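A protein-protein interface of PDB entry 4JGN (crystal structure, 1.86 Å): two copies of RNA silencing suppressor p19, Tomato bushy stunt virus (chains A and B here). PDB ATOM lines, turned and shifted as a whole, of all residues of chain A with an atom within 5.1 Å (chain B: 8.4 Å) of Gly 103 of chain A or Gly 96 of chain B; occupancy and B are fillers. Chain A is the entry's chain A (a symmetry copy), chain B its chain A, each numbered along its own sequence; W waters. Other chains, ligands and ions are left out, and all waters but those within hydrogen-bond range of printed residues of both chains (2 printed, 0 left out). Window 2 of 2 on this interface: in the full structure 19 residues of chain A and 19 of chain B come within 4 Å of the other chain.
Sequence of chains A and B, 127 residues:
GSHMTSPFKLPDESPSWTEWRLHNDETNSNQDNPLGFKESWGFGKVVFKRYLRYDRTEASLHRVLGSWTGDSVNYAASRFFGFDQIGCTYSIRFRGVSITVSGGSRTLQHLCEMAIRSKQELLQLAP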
ATOM      1  N   ILE A  86      14.328  -9.546  19.197  1.00  0.00           N
ATOM      2  CA  ILE A  86      15.074 -10.665  18.594  1.00  0.00           C
ATOM      3  C   ILE A  86      14.715 -10.680  17.087  1.00  0.00           C
ATOM      4  O   ILE A  86      13.701 -10.133  16.716  1.00  0.00           O
ATOM      5  CB  ILE A  86      14.640 -11.993  19.266  1.00  0.00           C
ATOM      6  CG1 ILE A  86      13.153 -12.292  19.070  1.00  0.00           C
ATOM      7  CG2 ILE A  86      15.030 -11.957  20.847  1.00  0.00           C
ATOM      8  CD1 ILE A  86      12.791 -13.737  19.575  1.00  0.00           C
ATOM      9  N   GLY A  87      15.490 -11.353  16.263  1.00  0.00           N
ATOM     10  CA  GLY A  87      15.051 -11.466  14.847  1.00  0.00           C
ATOM     11  C   GLY A  87      14.060 -12.599  14.638  1.00  0.00           C
ATOM     12  O   GLY A  87      14.173 -13.714  15.218  1.00  0.00           O
ATOM     13  N   CYS A  88      13.101 -12.324  13.763  1.00  0.00           N
ATOM     14  CA  CYS A  88      12.076 -13.264  13.413  1.00  0.00           C
ATOM     15  C   CYS A  88      12.077 -13.426  11.909  1.00  0.00           C
ATOM     16  O   CYS A  88      12.179 -12.408  11.149  1.00  0.00           O
ATOM     17  CB  CYS A  88      10.765 -12.692  13.767  1.00  0.00           C
ATOM     18  SG  CYS A  88      10.578 -12.518  15.662  1.00  0.00           S
ATOM     19  N   VAL A 101      10.637 -13.593   4.861  1.00  0.00           N
ATOM     20  CA  VAL A 101      10.127 -12.326   5.327  1.00  0.00           C
ATOM     21  C   VAL A 101      10.743 -12.192   6.711  1.00  0.00           C
ATOM     22  O   VAL A 101      10.605 -13.115   7.587  1.00  0.00           O
ATOM     23  CB  VAL A 101       8.615 -12.407   5.473  1.00  0.00           C
ATOM     24  CG1 VAL A 101       8.109 -11.069   6.021  1.00  0.00           C
ATOM     25  CG2 VAL A 101       7.954 -12.674   4.083  1.00  0.00           C
ATOM     26  N   SER A 102      11.426 -11.105   6.974  1.00  0.00           N
ATOM     27  CA  SER A 102      12.171 -11.052   8.249  1.00  0.00           C
ATOM     28  C   SER A 102      12.226  -9.652   8.845  1.00  0.00           C
ATOM     29  O   SER A 102      12.106  -8.636   8.110  1.00  0.00           O
ATOM     30  CB  SER A 102      13.530 -11.729   8.076  1.00  0.00           C
ATOM     31  OG  SER A 102      14.377 -11.017   7.269  1.00  0.00           O
ATOM     32  N   GLY A 103      12.400  -9.581  10.188  1.00  0.00           N
ATOM     33  CA  GLY A 103      12.602  -8.284  10.818  1.00  0.00           C
ATOM     34  C   GLY A 103      12.613  -8.545  12.330  1.00  0.00           C
ATOM     35  O   GLY A 103      12.764  -9.715  12.785  1.00  0.00           O
ATOM     36  N   GLY A 104      12.498  -7.487  13.086  1.00  0.00           N
ATOM     37  CA  GLY A 104      12.664  -7.671  14.532  1.00  0.00           C
ATOM     38  C   GLY A 104      11.312  -8.011  15.129  1.00  0.00           C
ATOM     39  O   GLY A 104      10.268  -7.734  14.560  1.00  0.00           O
ATOM     40  N   SER A 105      11.304  -8.488  16.390  1.00  0.00           N
ATOM     41  CA  SER A 105      10.016  -8.949  16.964  1.00  0.00           C
ATOM     42  C   SER A 105       9.023  -7.837  17.158  1.00  0.00           C
ATOM     43  O   SER A 105       7.814  -8.098  17.279  1.00  0.00           O
ATOM     44  CB  SER A 105      10.262  -9.674  18.302  1.00  0.00           C
ATOM     45  OG  SER A 105      11.271  -9.052  19.094  1.00  0.00           O
ATOM     46  N   THR A 107       8.173  -5.966  14.974  1.00  0.00           N
ATOM     47  CA  THR A 107       7.388  -5.881  13.699  1.00  0.00           C
ATOM     48  C   THR A 107       6.613  -7.173  13.377  1.00  0.00           C
ATOM     49  O   THR A 107       6.043  -7.325  12.300  1.00  0.00           O
ATOM     50  CB  THR A 107       8.345  -5.507  12.491  1.00  0.00           C
ATOM     51  OG1 THR A 107       9.144  -6.678  12.136  1.00  0.00           O
ATOM     52  CG2 THR A 107       9.243  -4.418  12.965  1.00  0.00           C
ATOM     53  N   LEU A 111       5.217  -8.692   9.870  1.00  0.00           N
ATOM     54  CA  LEU A 111       5.849  -9.876   9.294  1.00  0.00           C
ATOM     55  C   LEU A 111       4.800 -10.957   8.948  1.00  0.00           C
ATOM     56  O   LEU A 111       4.850 -11.501   7.892  1.00  0.00           O
ATOM     57  CB  LEU A 111       6.900 -10.464  10.214  1.00  0.00           C
ATOM     58  CG  LEU A 111       8.055  -9.573  10.637  1.00  0.00           C
ATOM     59  CD1 LEU A 111       9.020 -10.331  11.605  1.00  0.00           C
ATOM     60  CD2 LEU A 111       8.864  -9.049   9.384  1.00  0.00           C
ATOM     61  N   ASN B  30      10.502   7.949  12.616  1.00  0.00           N
ATOM     62  CA  ASN B  30      11.107   7.823  11.283  1.00  0.00           C
ATOM     63  C   ASN B  30      11.315   6.378  10.792  1.00  0.00           C
ATOM     64  O   ASN B  30      11.781   6.164   9.659  1.00  0.00           O
ATOM     65  CB  ASN B  30      12.381   8.670  11.172  1.00  0.00           C
ATOM     66  CG  ASN B  30      13.449   8.226  12.120  1.00  0.00           C
ATOM     67  OD1 ASN B  30      13.869   7.078  12.091  1.00  0.00           O
ATOM     68  ND2 ASN B  30      13.882   9.123  12.983  1.00  0.00           N
ATOM     69  N   GLN B  31      10.948   5.388  11.626  1.00  0.00           N
ATOM     70  CA  GLN B  31      10.800   4.023  11.110  1.00  0.00           C
ATOM     71  C   GLN B  31       9.414   3.881  10.442  1.00  0.00           C
ATOM     72  O   GLN B  31       9.296   3.224   9.395  1.00  0.00           O
ATOM     73  CB  GLN B  31      11.119   2.999  12.192  1.00  0.00           C
ATOM     74  CG  GLN B  31      12.197   3.560  13.135  1.00  0.00           C
ATOM     75  CD  GLN B  31      12.896   2.517  13.985  1.00  0.00           C
ATOM     76  OE1 GLN B  31      13.829   2.857  14.719  1.00  0.00           O
ATOM     77  NE2 GLN B  31      12.461   1.245  13.893  1.00  0.00           N
ATOM     78  N   ASP B  32       8.418   4.594  10.990  1.00  0.00           N
ATOM     79  CA  ASP B  32       7.075   4.745  10.378  1.00  0.00           C
ATOM     80  C   ASP B  32       7.046   5.528   9.044  1.00  0.00           C
ATOM     81  O   ASP B  32       6.273   5.170   8.143  1.00  0.00           O
ATOM     82  CB  ASP B  32       6.107   5.430  11.361  1.00  0.00           C
ATOM     83  CG  ASP B  32       5.833   4.572  12.632  1.00  0.00           C
ATOM     84  OD1 ASP B  32       6.544   3.550  12.841  1.00  0.00           O
ATOM     85  OD2 ASP B  32       4.913   4.915  13.427  1.00  0.00           O
ATOM     86  N   PRO B  34       9.968   6.697   6.776  1.00  0.00           N
ATOM     87  CA  PRO B  34      11.301   6.796   6.210  1.00  0.00           C
ATOM     88  C   PRO B  34      11.284   7.647   4.952  1.00  0.00           C
ATOM     89  O   PRO B  34      10.229   7.862   4.388  1.00  0.00           O
ATOM     90  CB  PRO B  34      11.625   5.347   5.838  1.00  0.00           C
ATOM     91  CG  PRO B  34      10.278   4.748   5.635  1.00  0.00           C
ATOM     92  CD  PRO B  34       9.344   5.385   6.549  1.00  0.00           C
ATOM     93  N   GLY B  36      12.258   6.590   2.151  1.00  0.00           N
ATOM     94  CA  GLY B  36      11.930   5.646   1.066  1.00  0.00           C
ATOM     95  C   GLY B  36      12.331   4.223   1.513  1.00  0.00           C
ATOM     96  O   GLY B  36      12.283   3.868   2.729  1.00  0.00           O
ATOM     97  N   LYS B  38      14.764   0.423   0.462  1.00  0.00           N
ATOM     98  CA  LYS B  38      15.978  -0.044  -0.159  1.00  0.00           C
ATOM     99  C   LYS B  38      15.683  -1.362  -0.856  1.00  0.00           C
ATOM    100  O   LYS B  38      14.930  -2.170  -0.330  1.00  0.00           O
ATOM    101  CB  LYS B  38      17.029  -0.315   0.922  1.00  0.00           C
ATOM    102  CG  LYS B  38      17.247   0.883   1.844  1.00  0.00           C
ATOM    103  CD  LYS B  38      17.774   0.484   3.266  1.00  0.00           C
ATOM    104  CE  LYS B  38      17.797   1.698   4.334  1.00  0.00           C
ATOM    105  NZ  LYS B  38      16.523   2.296   5.061  1.00  0.00           N
ATOM    106  N   ILE B  92      14.154  -6.465  -0.503  1.00  0.00           N
ATOM    107  CA  ILE B  92      13.602  -5.160  -0.398  1.00  0.00           C
ATOM    108  C   ILE B  92      13.357  -4.993   1.150  1.00  0.00           C
ATOM    109  O   ILE B  92      12.935  -5.979   1.811  1.00  0.00           O
ATOM    110  CB  ILE B  92      12.249  -4.996  -1.223  1.00  0.00           C
ATOM    111  CG1 ILE B  92      11.731  -3.545  -1.061  1.00  0.00           C
ATOM    112  CG2 ILE B  92      11.190  -6.082  -0.846  1.00  0.00           C
ATOM    113  CD1 ILE B  92      10.512  -3.246  -1.961  1.00  0.00           C
ATOM    114  N   ARG B  93      13.662  -3.810   1.684  1.00  0.00           N
ATOM    115  CA  ARG B  93      13.331  -3.540   3.062  1.00  0.00           C
ATOM    116  C   ARG B  93      12.555  -2.219   3.142  1.00  0.00           C
ATOM    117  O   ARG B  93      13.026  -1.141   2.628  1.00  0.00           O
ATOM    118  CB  ARG B  93      14.621  -3.395   3.850  1.00  0.00           C
ATOM    119  CG  ARG B  93      14.318  -3.274   5.392  1.00  0.00           C
ATOM    120  CD  ARG B  93      15.571  -2.922   6.087  1.00  0.00           C
ATOM    121  NE  ARG B  93      15.251  -2.721   7.544  1.00  0.00           N
ATOM    122  CZ  ARG B  93      15.745  -3.441   8.554  1.00  0.00           C
ATOM    123  NH1 ARG B  93      16.649  -4.395   8.324  1.00  0.00           N
ATOM    124  NH2 ARG B  93      15.437  -3.110   9.844  1.00  0.00           N
ATOM    125  N   PHE B  94      11.474  -2.234   3.908  1.00  0.00           N
ATOM    126  CA  PHE B  94      10.663  -1.048   4.075  1.00  0.00           C
ATOM    127  C   PHE B  94       9.995  -1.102   5.443  1.00  0.00           C
ATOM    128  O   PHE B  94       9.350  -2.121   5.789  1.00  0.00           O
ATOM    129  CB  PHE B  94       9.592  -0.961   2.980  1.00  0.00           C
ATOM    130  CG  PHE B  94       8.754   0.295   3.053  1.00  0.00           C
ATOM    131  CD1 PHE B  94       9.367   1.565   3.053  1.00  0.00           C
ATOM    132  CD2 PHE B  94       7.328   0.218   3.035  1.00  0.00           C
ATOM    133  CE1 PHE B  94       8.575   2.738   3.110  1.00  0.00           C
ATOM    134  CE2 PHE B  94       6.512   1.405   3.050  1.00  0.00           C
ATOM    135  CZ  PHE B  94       7.139   2.663   3.064  1.00  0.00           C
ATOM    136  N   ARG B  95      10.179  -0.013   6.212  1.00  0.00           N
ATOM    137  CA  ARG B  95       9.603   0.039   7.561  1.00  0.00           C
ATOM    138  C   ARG B  95       9.890  -1.208   8.403  1.00  0.00           C
ATOM    139  O   ARG B  95       8.986  -1.780   8.977  1.00  0.00           O
ATOM    140  CB  ARG B  95       8.134   0.189   7.458  1.00  0.00           C
ATOM    141  CG  ARG B  95       7.731   1.525   6.917  1.00  0.00           C
ATOM    142  CD  ARG B  95       6.273   1.325   6.584  1.00  0.00           C
ATOM    143  NE  ARG B  95       5.554   2.566   6.647  1.00  0.00           N
ATOM    144  CZ  ARG B  95       4.248   2.651   6.437  1.00  0.00           C
ATOM    145  NH1 ARG B  95       3.551   1.534   6.167  1.00  0.00           N
ATOM    146  NH2 ARG B  95       3.657   3.844   6.502  1.00  0.00           N
ATOM    147  N   GLY B  96      11.137  -1.569   8.514  1.00  0.00           N
ATOM    148  CA  GLY B  96      11.495  -2.618   9.431  1.00  0.00           C
ATOM    149  C   GLY B  96      11.253  -4.079   8.938  1.00  0.00           C
ATOM    150  O   GLY B  96      11.590  -5.002   9.692  1.00  0.00           O
ATOM    151  N   VAL B  97      10.632  -4.277   7.756  1.00  0.00           N
ATOM    152  CA  VAL B  97      10.371  -5.590   7.240  1.00  0.00           C
ATOM    153  C   VAL B  97      11.170  -5.828   5.953  1.00  0.00           C
ATOM    154  O   VAL B  97      11.169  -4.965   5.091  1.00  0.00           O
ATOM    155  CB  VAL B  97       8.881  -5.870   6.947  1.00  0.00           C
ATOM    156  CG1 VAL B  97       7.947  -5.555   8.159  1.00  0.00           C
ATOM    157  CG2 VAL B  97       8.458  -5.155   5.862  1.00  0.00           C
ATOM    158  N   SER B  98      11.934  -6.911   5.928  1.00  0.00           N
ATOM    159  CA  SER B  98      12.623  -7.311   4.714  1.00  0.00           C
ATOM    160  C   SER B  98      11.980  -8.470   4.047  1.00  0.00           C
ATOM    161  O   SER B  98      11.663  -9.459   4.731  1.00  0.00           O
ATOM    162  CB  SER B  98      14.026  -7.788   5.005  1.00  0.00           C
ATOM    163  OG  SER B  98      14.576  -6.698   5.724  1.00  0.00           O
ATOM    164  N   ILE B  99      11.913  -8.434   2.711  1.00  0.00           N
ATOM    165  CA  ILE B  99      11.478  -9.652   1.992  1.00  0.00           C
ATOM    166  C   ILE B  99      12.644 -10.004   1.030  1.00  0.00           C
ATOM    167  O   ILE B  99      13.212  -9.107   0.380  1.00  0.00           O
ATOM    168  CB  ILE B  99      10.164  -9.391   1.173  1.00  0.00           C
ATOM    169  CG1 ILE B  99       9.055  -8.961   2.184  1.00  0.00           C
ATOM    170  CG2 ILE B  99       9.731 -10.699   0.357  1.00  0.00           C
ATOM    171  CD1 ILE B  99       7.589  -8.670   1.496  1.00  0.00           C
ATOM    172  N   LEU B 122       4.510  -5.116  -0.103  1.00  0.00           N
ATOM    173  CA  LEU B 122       5.176  -4.469   0.993  1.00  0.00           C
ATOM    174  C   LEU B 122       5.021  -2.941   0.987  1.00  0.00           C
ATOM    175  O   LEU B 122       4.787  -2.301   2.026  1.00  0.00           O
ATOM    176  CB  LEU B 122       6.676  -4.821   0.947  1.00  0.00           C
ATOM    177  CG  LEU B 122       7.484  -4.224   2.111  1.00  0.00           C
ATOM    178  CD1 LEU B 122       6.944  -4.710   3.500  1.00  0.00           C
ATOM    179  CD2 LEU B 122       8.955  -4.593   1.942  1.00  0.00           C
HETATM  180  O   HOH W   1      12.885  -4.949  11.864  1.00  0.00           O
HETATM  181  O   HOH W   2      13.877 -11.523   4.579  1.00  0.00           O
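Of the 15 printed residues of chain B, 3 touch a printed residue of chain A. Hydrophobic or aromatic side chains of chain B within 4 Å of the printed part of chain A: Val 97. Of the 10 printed residues of chain A, 5 touch a printed residue of chain B. Printed residues of chain A that touch a printed residue of chain B: Val 101, Ser 102, Gly 103, Thr 107 and Leu 111. Hydrophobic or aromatic side chains of chain A that line the printed part of chain B: Leu 111. Among the printed residues, no Asp or Glu carboxylate lies within 4 Å of a Lys or Arg side-chain nitrogen of the other chain.
Printed residues of chain B within 4 Å of Val 101 of chain A: Ser 98. Printed residues of chain B within 4 Å of Ser 102 of chain A: Gly 96 (3.997 Å), Val 97 (3.6 Å) and Ser 98 (2.8 Å). Of chain B, only Gly 96 (3.6 Å) comes within 4 Å of Gly 103 of chain A. No residue of chain B comes within 4 Å of Gly 104 of chain A. Of the printed residues of chain B, Thr 107 of chain A touches Gly 96 (3.8 Å). Gln 31 of chain B touches none of the printed residues of chain A. Lys 38 of chain B touches none of the printed residues of chain A. Printed residues of chain A within 4 Å of Gly 96 of chain B: Ser 102 (3.997 Å), Gly 103 (3.6 Å) and Thr 107 (3.8 Å). The nearest printed residue of chain B that does not touch Leu 111 of chain A is Gly 96 of chain B (4.9 Å).
Water W1 bridges the backbone carbonyl oxygen of Gly 96 of chain B and the backbone NH of Gly 104 of chain A. Water W2 lies within hydrogen-bond range of the side-chain hydroxyl (OG) of Ser 102 of chain A (2.8 Å) and the backbone carbonyl oxygen (O) of Ser 98 of chain B (3.0 Å).
Among the printed residues, merely in contact across the chains: Val 101 of chain A with Ser 98 of chain B (3.3 Å), Ser 102 of chain A with Val 97 of chain B (3.6 Å), Gly 103 of chain A with Gly 96 of chain B (3.6 Å), Leu 111 of chain A with Val 97 of chain B (3.8 Å), Thr 107 of chain A with Gly 96 of chain B (3.8 Å) and Ser 102 of chain A with Gly 96 of chain B (3.997 Å).
No position is printed for both chains. Of the 7 pairs that touch across the chains among the printed residues, none has its exchanged pair printed and touching as well.
N of Cys 88 of chain A sits at hydrogen-bond distance from O of Gly 103 of chain A, 2.8 Å away. O of Gly 104 of chain A sits at hydrogen-bond distance from OG1 of Thr 107 of chain A, at 2.9 Å.
The backbone carbonyl oxygen (O) of Ser 102 of chain A lies within hydrogen-bond range of the backbone NH (N) of Ser 98 of chain B (2.8 Å).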
